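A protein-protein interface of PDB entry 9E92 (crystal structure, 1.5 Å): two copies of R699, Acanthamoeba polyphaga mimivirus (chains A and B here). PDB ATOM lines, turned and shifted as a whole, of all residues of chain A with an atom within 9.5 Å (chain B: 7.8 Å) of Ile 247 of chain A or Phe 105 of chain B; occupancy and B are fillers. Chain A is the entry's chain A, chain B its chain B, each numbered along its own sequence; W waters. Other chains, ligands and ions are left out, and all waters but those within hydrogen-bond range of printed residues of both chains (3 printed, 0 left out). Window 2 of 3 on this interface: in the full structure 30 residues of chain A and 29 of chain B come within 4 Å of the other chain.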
ATOM      1  N   ASP A 241      23.184 -19.150 -19.591  1.00  0.00           N
ATOM      2  CA  ASP A 241      22.187 -18.903 -20.620  1.00  0.00           C
ATOM      3  C   ASP A 241      20.987 -19.810 -20.365  1.00  0.00           C
ATOM      4  O   ASP A 241      21.023 -21.030 -20.613  1.00  0.00           O
ATOM      5  CB  ASP A 241      22.727 -19.222 -21.989  1.00  0.00           C
ATOM      6  CG  ASP A 241      21.684 -19.104 -23.087  1.00  0.00           C
ATOM      7  OD1 ASP A 241      20.577 -18.614 -22.805  1.00  0.00           O
ATOM      8  OD2 ASP A 241      22.020 -19.530 -24.217  1.00  0.00           O
ATOM      9  N   GLY A 242      19.962 -19.245 -19.726  1.00  0.00           N
ATOM     10  CA  GLY A 242      18.804 -20.004 -19.362  1.00  0.00           C
ATOM     11  C   GLY A 242      18.064 -20.605 -20.532  1.00  0.00           C
ATOM     12  O   GLY A 242      17.298 -21.536 -20.297  1.00  0.00           O
ATOM     13  N   SER A 243      18.266 -20.150 -21.785  1.00  0.00           N
ATOM     14  CA  SER A 243      17.621 -20.749 -22.950  1.00  0.00           C
ATOM     15  C   SER A 243      18.466 -21.858 -23.607  1.00  0.00           C
ATOM     16  O   SER A 243      18.111 -22.343 -24.674  1.00  0.00           O
ATOM     17  CB  SER A 243      17.247 -19.673 -23.945  1.00  0.00           C
ATOM     18  OG  SER A 243      18.408 -19.108 -24.526  1.00  0.00           O
ATOM     19  N   SER A 244      19.512 -22.328 -22.919  1.00  0.00           N
ATOM     20  CA  SER A 244      20.456 -23.313 -23.486  1.00  0.00           C
ATOM     21  C   SER A 244      19.764 -24.579 -23.997  1.00  0.00           C
ATOM     22  O   SER A 244      20.158 -25.069 -25.072  1.00  0.00           O
ATOM     23  CB  SER A 244      21.567 -23.638 -22.493  1.00  0.00           C
ATOM     24  OG  SER A 244      21.058 -24.256 -21.322  1.00  0.00           O
ATOM     25  N   ASN A 245      18.735 -25.078 -23.299  1.00  0.00           N
ATOM     26  CA  ASN A 245      18.014 -26.289 -23.713  1.00  0.00           C
ATOM     27  C   ASN A 245      16.556 -26.039 -24.127  1.00  0.00           C
ATOM     28  O   ASN A 245      15.783 -26.994 -24.279  1.00  0.00           O
ATOM     29  CB  ASN A 245      18.049 -27.377 -22.645  1.00  0.00           C
ATOM     30  CG  ASN A 245      18.077 -28.781 -23.225  1.00  0.00           C
ATOM     31  OD1 ASN A 245      18.967 -29.081 -24.034  1.00  0.00           O
ATOM     32  ND2 ASN A 245      17.136 -29.601 -22.806  1.00  0.00           N
ATOM     33  N   THR A 246      16.168 -24.751 -24.357  1.00  0.00           N
ATOM     34  CA  THR A 246      14.787 -24.445 -24.738  1.00  0.00           C
ATOM     35  C   THR A 246      14.461 -25.174 -26.050  1.00  0.00           C
ATOM     36  O   THR A 246      13.359 -25.705 -26.199  1.00  0.00           O
ATOM     37  CB  THR A 246      14.635 -22.918 -24.871  1.00  0.00           C
ATOM     38  OG1 THR A 246      14.852 -22.314 -23.597  1.00  0.00           O
ATOM     39  CG2 THR A 246      13.258 -22.494 -25.341  1.00  0.00           C
ATOM     40  N   ILE A 247      15.417 -25.139 -26.977  1.00  0.00           N
ATOM     41  CA  ILE A 247      15.484 -26.002 -28.157  1.00  0.00           C
ATOM     42  C   ILE A 247      16.483 -27.121 -27.853  1.00  0.00           C
ATOM     43  O   ILE A 247      17.657 -26.846 -27.611  1.00  0.00           O
ATOM     44  CB  ILE A 247      15.896 -25.216 -29.412  1.00  0.00           C
ATOM     45  CG1 ILE A 247      14.920 -24.059 -29.712  1.00  0.00           C
ATOM     46  CG2 ILE A 247      16.070 -26.149 -30.629  1.00  0.00           C
ATOM     47  CD1 ILE A 247      15.474 -23.031 -30.696  1.00  0.00           C
ATOM     48  N   ASN A 248      16.032 -28.370 -27.913  1.00  0.00           N
ATOM     49  CA  ASN A 248      16.906 -29.487 -27.530  1.00  0.00           C
ATOM     50  C   ASN A 248      17.282 -30.397 -28.702  1.00  0.00           C
ATOM     51  O   ASN A 248      17.641 -31.560 -28.494  1.00  0.00           O
ATOM     52  CB  ASN A 248      16.318 -30.217 -26.339  1.00  0.00           C
ATOM     53  CG  ASN A 248      15.187 -31.128 -26.700  1.00  0.00           C
ATOM     54  OD1 ASN A 248      14.590 -31.019 -27.766  1.00  0.00           O
ATOM     55  ND2 ASN A 248      14.922 -32.077 -25.837  1.00  0.00           N
ATOM     56  N   THR A 249      17.254 -29.860 -29.931  1.00  0.00           N
ATOM     57  CA  THR A 249      17.815 -30.475 -31.131  1.00  0.00           C
ATOM     58  C   THR A 249      19.106 -29.725 -31.483  1.00  0.00           C
ATOM     59  O   THR A 249      19.199 -28.514 -31.302  1.00  0.00           O
ATOM     60  CB  THR A 249      16.799 -30.405 -32.276  1.00  0.00           C
ATOM     61  OG1 THR A 249      16.483 -29.033 -32.487  1.00  0.00           O
ATOM     62  CG2 THR A 249      15.539 -31.169 -31.952  1.00  0.00           C
ATOM     63  N   PHE A 250      20.097 -30.433 -31.999  1.00  0.00           N
ATOM     64  CA  PHE A 250      21.420 -29.904 -32.247  1.00  0.00           C
ATOM     65  C   PHE A 250      21.918 -30.383 -33.607  1.00  0.00           C
ATOM     66  O   PHE A 250      21.845 -31.577 -33.909  1.00  0.00           O
ATOM     67  CB  PHE A 250      22.379 -30.373 -31.140  1.00  0.00           C
ATOM     68  CG  PHE A 250      21.907 -29.952 -29.756  1.00  0.00           C
ATOM     69  CD1 PHE A 250      22.275 -28.728 -29.210  1.00  0.00           C
ATOM     70  CD2 PHE A 250      21.051 -30.762 -29.003  1.00  0.00           C
ATOM     71  CE1 PHE A 250      21.797 -28.324 -27.964  1.00  0.00           C
ATOM     72  CE2 PHE A 250      20.582 -30.366 -27.762  1.00  0.00           C
ATOM     73  CZ  PHE A 250      20.957 -29.149 -27.226  1.00  0.00           C
ATOM     74  N   LYS A 251      22.570 -29.484 -34.372  1.00  0.00           N
ATOM     75  CA  LYS A 251      23.111 -29.818 -35.682  1.00  0.00           C
ATOM     76  C   LYS A 251      24.323 -28.932 -36.009  1.00  0.00           C
ATOM     77  O   LYS A 251      24.195 -27.691 -36.039  1.00  0.00           O
ATOM     78  CB  LYS A 251      22.061 -29.566 -36.773  1.00  0.00           C
ATOM     79  CG  LYS A 251      22.570 -29.930 -38.168  1.00  0.00           C
ATOM     80  CD  LYS A 251      21.500 -29.716 -39.234  1.00  0.00           C
ATOM     81  CE  LYS A 251      21.974 -30.207 -40.575  1.00  0.00           C
ATOM     82  NZ  LYS A 251      22.180 -31.658 -40.584  1.00  0.00           N
ATOM     83  N   LYS A 342      19.060 -40.909 -28.494  1.00  0.00           N
ATOM     84  CA  LYS A 342      19.011 -39.535 -28.957  1.00  0.00           C
ATOM     85  C   LYS A 342      19.856 -39.400 -30.228  1.00  0.00           C
ATOM     86  O   LYS A 342      21.085 -39.335 -30.174  1.00  0.00           O
ATOM     87  CB  LYS A 342      19.395 -38.570 -27.837  1.00  0.00           C
ATOM     88  CG  LYS A 342      19.066 -37.079 -28.211  1.00  0.00           C
ATOM     89  CD  LYS A 342      19.172 -36.119 -27.041  1.00  0.00           C
ATOM     90  CE  LYS A 342      18.567 -34.756 -27.258  1.00  0.00           C
ATOM     91  NZ  LYS A 342      19.399 -33.914 -28.108  1.00  0.00           N
ATOM     92  N   ASP A 344      20.693 -37.143 -32.464  1.00  0.00           N
ATOM     93  CA  ASP A 344      21.596 -36.013 -32.661  1.00  0.00           C
ATOM     94  C   ASP A 344      22.667 -35.862 -31.584  1.00  0.00           C
ATOM     95  O   ASP A 344      23.292 -34.787 -31.458  1.00  0.00           O
ATOM     96  CB  ASP A 344      20.818 -34.714 -32.801  1.00  0.00           C
ATOM     97  CG  ASP A 344      20.086 -34.259 -31.557  1.00  0.00           C
ATOM     98  OD1 ASP A 344      20.131 -35.001 -30.557  1.00  0.00           O
ATOM     99  OD2 ASP A 344      19.339 -33.251 -31.623  1.00  0.00           O
ATOM    100  N   GLU A 348      25.234 -32.615 -30.213  1.00  0.00           N
ATOM    101  CA  GLU A 348      25.064 -32.035 -28.880  1.00  0.00           C
ATOM    102  C   GLU A 348      26.389 -32.062 -28.096  1.00  0.00           C
ATOM    103  O   GLU A 348      26.753 -31.088 -27.430  1.00  0.00           O
ATOM    104  CB  GLU A 348      23.954 -32.776 -28.135  1.00  0.00           C
ATOM    105  CG  GLU A 348      23.640 -32.185 -26.768  1.00  0.00           C
ATOM    106  CD  GLU A 348      22.476 -32.819 -26.009  1.00  0.00           C
ATOM    107  OE1 GLU A 348      21.723 -33.616 -26.637  1.00  0.00           O
ATOM    108  OE2 GLU A 348      22.366 -32.480 -24.800  1.00  0.00           O
ATOM    109  N   MET A 351      29.360 -29.751 -29.385  1.00  0.00           N
ATOM    110  CA  MET A 351      29.111 -28.362 -29.024  1.00  0.00           C
ATOM    111  C   MET A 351      29.565 -28.006 -27.601  1.00  0.00           C
ATOM    112  O   MET A 351      29.743 -26.823 -27.303  1.00  0.00           O
ATOM    113  CB  MET A 351      27.641 -27.973 -29.223  1.00  0.00           C
ATOM    114  CG  MET A 351      27.261 -27.939 -30.703  1.00  0.00           C
ATOM    115  SD  MET A 351      25.511 -27.533 -30.902  1.00  0.00           S
ATOM    116  CE  MET A 351      25.363 -27.804 -32.670  1.00  0.00           C
ATOM    117  N   ASN A 451      22.088 -33.253 -19.686  1.00  0.00           N
ATOM    118  CA  ASN A 451      21.221 -32.176 -20.192  1.00  0.00           C
ATOM    119  C   ASN A 451      19.922 -32.688 -20.793  1.00  0.00           C
ATOM    120  O   ASN A 451      18.954 -31.937 -20.913  1.00  0.00           O
ATOM    121  CB  ASN A 451      21.961 -31.232 -21.134  1.00  0.00           C
ATOM    122  CG  ASN A 451      22.870 -30.288 -20.410  1.00  0.00           C
ATOM    123  OD1 ASN A 451      22.783 -30.119 -19.188  1.00  0.00           O
ATOM    124  ND2 ASN A 451      23.821 -29.714 -21.137  1.00  0.00           N
ATOM    125  N   ASN A 452      19.923 -33.920 -21.297  1.00  0.00           N
ATOM    126  CA  ASN A 452      18.809 -34.501 -22.021  1.00  0.00           C
ATOM    127  C   ASN A 452      18.731 -36.017 -21.792  1.00  0.00           C
ATOM    128  O   ASN A 452      19.532 -36.601 -21.055  1.00  0.00           O
ATOM    129  CB  ASN A 452      18.936 -34.197 -23.516  1.00  0.00           C
ATOM    130  CG  ASN A 452      18.570 -32.771 -23.883  1.00  0.00           C
ATOM    131  OD1 ASN A 452      17.394 -32.391 -23.747  1.00  0.00           O
ATOM    132  ND2 ASN A 452      19.541 -31.974 -24.249  1.00  0.00           N
ATOM    133  N   ILE B  99      14.815 -13.413 -22.607  1.00  0.00           N
ATOM    134  CA  ILE B  99      13.361 -13.267 -22.680  1.00  0.00           C
ATOM    135  C   ILE B  99      12.905 -13.310 -24.150  1.00  0.00           C
ATOM    136  O   ILE B  99      11.942 -14.024 -24.494  1.00  0.00           O
ATOM    137  CB  ILE B  99      12.874 -11.982 -21.993  1.00  0.00           C
ATOM    138  CG1 ILE B  99      13.091 -12.088 -20.469  1.00  0.00           C
ATOM    139  CG2 ILE B  99      11.402 -11.714 -22.292  1.00  0.00           C
ATOM    140  CD1 ILE B  99      12.984 -10.750 -19.750  1.00  0.00           C
ATOM    141  N   LEU B 100      13.576 -12.523 -25.020  1.00  0.00           N
ATOM    142  CA  LEU B 100      13.159 -12.457 -26.418  1.00  0.00           C
ATOM    143  C   LEU B 100      13.432 -13.765 -27.147  1.00  0.00           C
ATOM    144  O   LEU B 100      12.560 -14.208 -27.909  1.00  0.00           O
ATOM    145  CB  LEU B 100      13.871 -11.299 -27.113  1.00  0.00           C
ATOM    146  CG  LEU B 100      13.448  -9.915 -26.644  1.00  0.00           C
ATOM    147  CD1 LEU B 100      14.404  -8.813 -27.067  1.00  0.00           C
ATOM    148  CD2 LEU B 100      12.063  -9.655 -27.108  1.00  0.00           C
ATOM    149  N   ARG B 101      14.560 -14.441 -26.899  1.00  0.00           N
ATOM    150  CA  ARG B 101      14.776 -15.758 -27.473  1.00  0.00           C
ATOM    151  C   ARG B 101      13.616 -16.700 -27.131  1.00  0.00           C
ATOM    152  O   ARG B 101      13.112 -17.458 -27.951  1.00  0.00           O
ATOM    153  CB  ARG B 101      16.099 -16.419 -27.072  1.00  0.00           C
ATOM    154  CG  ARG B 101      17.326 -15.743 -27.658  1.00  0.00           C
ATOM    155  CD  ARG B 101      18.630 -16.530 -27.396  1.00  0.00           C
ATOM    156  NE  ARG B 101      18.961 -16.560 -25.963  1.00  0.00           N
ATOM    157  CZ  ARG B 101      19.808 -15.744 -25.293  1.00  0.00           C
ATOM    158  NH1 ARG B 101      20.254 -14.649 -25.872  1.00  0.00           N
ATOM    159  NH2 ARG B 101      20.127 -15.978 -24.012  1.00  0.00           N
ATOM    160  N   LYS B 102      13.244 -16.717 -25.846  1.00  0.00           N
ATOM    161  CA  LYS B 102      12.197 -17.634 -25.417  1.00  0.00           C
ATOM    162  C   LYS B 102      10.829 -17.283 -26.017  1.00  0.00           C
ATOM    163  O   LYS B 102      10.107 -18.199 -26.401  1.00  0.00           O
ATOM    164  CB  LYS B 102      12.193 -17.640 -23.877  1.00  0.00           C
ATOM    165  CG  LYS B 102      13.307 -18.462 -23.237  1.00  0.00           C
ATOM    166  CD  LYS B 102      13.372 -18.356 -21.704  1.00  0.00           C
ATOM    167  CE  LYS B 102      14.304 -19.344 -21.135  1.00  0.00           C
ATOM    168  NZ  LYS B 102      14.349 -19.379 -19.661  1.00  0.00           N
ATOM    169  N   TYR B 103      10.452 -16.000 -26.013  1.00  0.00           N
ATOM    170  CA  TYR B 103       9.184 -15.559 -26.593  1.00  0.00           C
ATOM    171  C   TYR B 103       9.076 -16.030 -28.045  1.00  0.00           C
ATOM    172  O   TYR B 103       8.057 -16.627 -28.427  1.00  0.00           O
ATOM    173  CB  TYR B 103       9.031 -14.049 -26.466  1.00  0.00           C
ATOM    174  CG  TYR B 103       7.746 -13.534 -27.120  1.00  0.00           C
ATOM    175  CD1 TYR B 103       6.519 -13.621 -26.496  1.00  0.00           C
ATOM    176  CD2 TYR B 103       7.775 -13.032 -28.409  1.00  0.00           C
ATOM    177  CE1 TYR B 103       5.345 -13.188 -27.090  1.00  0.00           C
ATOM    178  CE2 TYR B 103       6.620 -12.559 -29.004  1.00  0.00           C
ATOM    179  CZ  TYR B 103       5.409 -12.623 -28.352  1.00  0.00           C
ATOM    180  OH  TYR B 103       4.250 -12.232 -28.966  1.00  0.00           O
ATOM    181  N   ARG B 104      10.130 -15.807 -28.831  1.00  0.00           N
ATOM    182  CA  ARG B 104      10.128 -16.176 -30.252  1.00  0.00           C
ATOM    183  C   ARG B 104       9.952 -17.677 -30.448  1.00  0.00           C
ATOM    184  O   ARG B 104       9.298 -18.108 -31.400  1.00  0.00           O
ATOM    185  CB  ARG B 104      11.441 -15.766 -30.933  1.00  0.00           C
ATOM    186  CG  ARG B 104      11.487 -14.258 -31.128  1.00  0.00           C
ATOM    187  CD  ARG B 104      12.660 -13.778 -31.935  1.00  0.00           C
ATOM    188  NE  ARG B 104      13.956 -13.848 -31.267  1.00  0.00           N
ATOM    189  CZ  ARG B 104      14.687 -12.855 -30.742  1.00  0.00           C
ATOM    190  NH1 ARG B 104      14.269 -11.590 -30.752  1.00  0.00           N
ATOM    191  NH2 ARG B 104      15.842 -13.163 -30.217  1.00  0.00           N
ATOM    192  N   PHE B 105      10.559 -18.492 -29.590  1.00  0.00           N
ATOM    193  CA  PHE B 105      10.425 -19.931 -29.673  1.00  0.00           C
ATOM    194  C   PHE B 105       8.990 -20.351 -29.298  1.00  0.00           C
ATOM    195  O   PHE B 105       8.402 -21.233 -29.939  1.00  0.00           O
ATOM    196  CB  PHE B 105      11.462 -20.642 -28.783  1.00  0.00           C
ATOM    197  CG  PHE B 105      11.202 -22.131 -28.670  1.00  0.00           C
ATOM    198  CD1 PHE B 105      11.547 -23.001 -29.699  1.00  0.00           C
ATOM    199  CD2 PHE B 105      10.539 -22.647 -27.556  1.00  0.00           C
ATOM    200  CE1 PHE B 105      11.291 -24.376 -29.579  1.00  0.00           C
ATOM    201  CE2 PHE B 105      10.278 -24.002 -27.463  1.00  0.00           C
ATOM    202  CZ  PHE B 105      10.672 -24.864 -28.456  1.00  0.00           C
ATOM    203  N   LEU B 106       8.454 -19.770 -28.212  1.00  0.00           N
ATOM    204  CA  LEU B 106       7.148 -20.164 -27.690  1.00  0.00           C
ATOM    205  C   LEU B 106       6.008 -19.821 -28.657  1.00  0.00           C
ATOM    206  O   LEU B 106       4.960 -20.493 -28.642  1.00  0.00           O
ATOM    207  CB  LEU B 106       6.921 -19.506 -26.321  1.00  0.00           C
ATOM    208  CG  LEU B 106       7.775 -20.035 -25.168  1.00  0.00           C
ATOM    209  CD1 LEU B 106       7.556 -19.217 -23.911  1.00  0.00           C
ATOM    210  CD2 LEU B 106       7.512 -21.484 -24.920  1.00  0.00           C
ATOM    211  N   THR B 107       6.125 -18.691 -29.359  1.00  0.00           N
ATOM    212  CA  THR B 107       5.049 -18.235 -30.256  1.00  0.00           C
ATOM    213  C   THR B 107       5.640 -17.596 -31.520  1.00  0.00           C
ATOM    214  O   THR B 107       5.800 -16.386 -31.650  1.00  0.00           O
ATOM    215  CB  THR B 107       4.054 -17.334 -29.528  1.00  0.00           C
ATOM    216  OG1 THR B 107       3.014 -17.013 -30.476  1.00  0.00           O
ATOM    217  CG2 THR B 107       4.610 -16.049 -28.938  1.00  0.00           C
ATOM    218  N   PRO B 108       5.941 -18.423 -32.549  1.00  0.00           N
ATOM    219  CA  PRO B 108       6.443 -17.875 -33.819  1.00  0.00           C
ATOM    220  C   PRO B 108       5.480 -16.881 -34.467  1.00  0.00           C
ATOM    221  O   PRO B 108       5.922 -15.994 -35.200  1.00  0.00           O
ATOM    222  CB  PRO B 108       6.703 -19.173 -34.650  1.00  0.00           C
ATOM    223  CG  PRO B 108       6.829 -20.272 -33.631  1.00  0.00           C
ATOM    224  CD  PRO B 108       5.878 -19.888 -32.506  1.00  0.00           C
ATOM    225  N   ASP B 109       4.175 -16.984 -34.159  1.00  0.00           N
ATOM    226  CA  ASP B 109       3.204 -16.051 -34.737  1.00  0.00           C
ATOM    227  C   ASP B 109       2.772 -14.933 -33.787  1.00  0.00           C
ATOM    228  O   ASP B 109       1.728 -14.289 -33.989  1.00  0.00           O
ATOM    229  CB  ASP B 109       1.989 -16.745 -35.314  1.00  0.00           C
ATOM    230  CG  ASP B 109       1.314 -17.790 -34.445  1.00  0.00           C
ATOM    231  OD1 ASP B 109       1.910 -18.215 -33.426  1.00  0.00           O
ATOM    232  OD2 ASP B 109       0.209 -18.214 -34.826  1.00  0.00           O
ATOM    233  N   VAL B 113       1.625 -14.689 -24.542  1.00  0.00           N
ATOM    234  CA  VAL B 113       2.032 -15.814 -23.711  1.00  0.00           C
ATOM    235  C   VAL B 113       1.723 -15.540 -22.239  1.00  0.00           C
ATOM    236  O   VAL B 113       2.198 -14.538 -21.698  1.00  0.00           O
ATOM    237  CB  VAL B 113       3.536 -16.154 -23.850  1.00  0.00           C
ATOM    238  CG1 VAL B 113       3.901 -17.371 -23.014  1.00  0.00           C
ATOM    239  CG2 VAL B 113       3.919 -16.392 -25.304  1.00  0.00           C
ATOM    240  N   VAL B 181      -1.306 -18.197 -25.737  1.00  0.00           N
ATOM    241  CA  VAL B 181      -0.556 -19.438 -25.571  1.00  0.00           C
ATOM    242  C   VAL B 181      -0.113 -19.558 -24.097  1.00  0.00           C
ATOM    243  O   VAL B 181       0.243 -18.521 -23.507  1.00  0.00           O
ATOM    244  CB  VAL B 181       0.665 -19.251 -26.515  1.00  0.00           C
ATOM    245  CG1 VAL B 181       1.817 -20.157 -26.180  1.00  0.00           C
ATOM    246  CG2 VAL B 181       0.226 -19.360 -27.985  1.00  0.00           C
ATOM    247  N   LYS B 185       5.960 -25.140 -20.068  1.00  0.00           N
ATOM    248  CA  LYS B 185       7.251 -25.633 -19.630  1.00  0.00           C
ATOM    249  C   LYS B 185       8.002 -24.636 -18.735  1.00  0.00           C
ATOM    250  O   LYS B 185       9.204 -24.825 -18.489  1.00  0.00           O
ATOM    251  CB  LYS B 185       8.121 -26.050 -20.830  1.00  0.00           C
ATOM    252  CG  LYS B 185       7.522 -27.259 -21.559  1.00  0.00           C
ATOM    253  CD  LYS B 185       8.484 -27.937 -22.530  1.00  0.00           C
ATOM    254  CE  LYS B 185       8.005 -29.355 -22.734  1.00  0.00           C
ATOM    255  NZ  LYS B 185       9.091 -30.309 -22.998  1.00  0.00           N
ATOM    256  N   GLU B 187       9.271 -21.653 -19.141  1.00  0.00           N
ATOM    257  CA  GLU B 187      10.456 -21.059 -19.747  1.00  0.00           C
ATOM    258  C   GLU B 187      10.532 -19.570 -19.379  1.00  0.00           C
ATOM    259  O   GLU B 187      11.603 -19.075 -18.984  1.00  0.00           O
ATOM    260  CB  GLU B 187      10.398 -21.263 -21.266  1.00  0.00           C
ATOM    261  CG  GLU B 187      10.599 -22.732 -21.622  1.00  0.00           C
ATOM    262  CD  GLU B 187      12.032 -23.197 -21.713  1.00  0.00           C
ATOM    263  OE1 GLU B 187      12.924 -22.361 -21.512  1.00  0.00           O
ATOM    264  OE2 GLU B 187      12.197 -24.437 -21.968  1.00  0.00           O
HETATM  265  O   HOH W   1      11.071 -25.685 -24.218  1.00  0.00           O
HETATM  266  O   HOH W   2      14.790 -22.258 -19.575  1.00  0.00           O
HETATM  267  O   HOH W   3      14.732 -25.335 -21.249  1.00  0.00           O
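NE of Arg 101 of chain B sits at hydrogen-bond distance from OG of Ser 243 of chain A, at 3.0 Å.
The side-chain carboxylate (OD1) of Asp 241 of chain A is in salt-bridge range of the guanidinium group (NH2) of Arg 101 of chain B (2.9 Å).
OG1 of Thr 246 of chain A is in hydrogen-bond range of OE1 of Glu 187 of chain B.
The side-chain amino group (NZ) of Lys 102 of chain B lies within salt-bridge range of the side-chain carboxylate (OE1) of Glu 187 of chain B (3.8 Å).
O of Ser 243 of chain A sits close to OG1 of Thr 246 of chain A, 3.4 Å away.
OG of Ser 244 of chain A sits close to O of Asp 241 of chain A.
OD1 of Asp 241 of chain A is in hydrogen-bond range of OG of Ser 243 of chain A (2.8 Å).
Among the printed residues, pairs that only touch across the chains: Thr 246 of chain A with Phe 105 of chain B (3.5 Å), Ile 247 of chain A with Phe 105 of chain B (3.5 Å), Gly 242 of chain A with Lys 102 of chain B (3.7 Å) and Thr 246 of chain A with Lys 102 of chain B (3.9 Å).
Of the printed residues of chain B, Ser 243 of chain A touches Arg 101 (3.0 Å).
Of chain B, only Phe 105 comes within 4 Å of Ile 247 of chain A.
Tyr 103 of chain B touches none of the printed residues of chain A.
Phe 105 of chain B touches two residues of chain A.
Printed residues of chain A within 4 Å of Glu 187 of chain B: Thr 246 (2.8 Å).
The nearest residue of chain B that does not touch Ile 247 of chain A is Glu 187 of chain B (6.0 Å).
The nearest printed residue of chain B that does not touch Gly 242 of chain A is Glu 187 of chain B (4.6 Å).
Of the 15 printed residues of chain B, 4 touch a printed residue of chain A.
Of the 17 printed residues of chain A, 5 touch a printed residue of chain B.
Printed residues of chain A that touch a printed residue of chain B: Asp 241, Gly 242, Ser 243, Thr 246 and Ile 247.
Among the printed residues, Asp or Glu carboxylates within 4 Å of a Lys or Arg side-chain nitrogen of the other chain: Asp 241 of chain A with Arg 101 of chain B (2.9 Å).
No position is printed for both chains.
Of the 7 pairs that touch across the chains among the printed residues, none has its exchanged pair printed and touching as well.
Water W2 lies within hydrogen-bond range of the side-chain carboxylate (OE1) of Glu 187 of chain B (2.7 Å), the backbone carbonyl oxygen (O) of Gly 242 of chain A (2.7 Å) and the side-chain amino group (NZ) of Lys 102 of chain B (2.9 Å).
Water W3 lies within hydrogen-bond range of the side-chain carboxylate (OE2) of Glu 187 of chain B (2.8 Å) and the backbone NH (N) of Thr 246 of chain A (3.5 Å).
Water W1 bridges OE2 of Glu 187 of chain B and O of Thr 246 of chain A.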
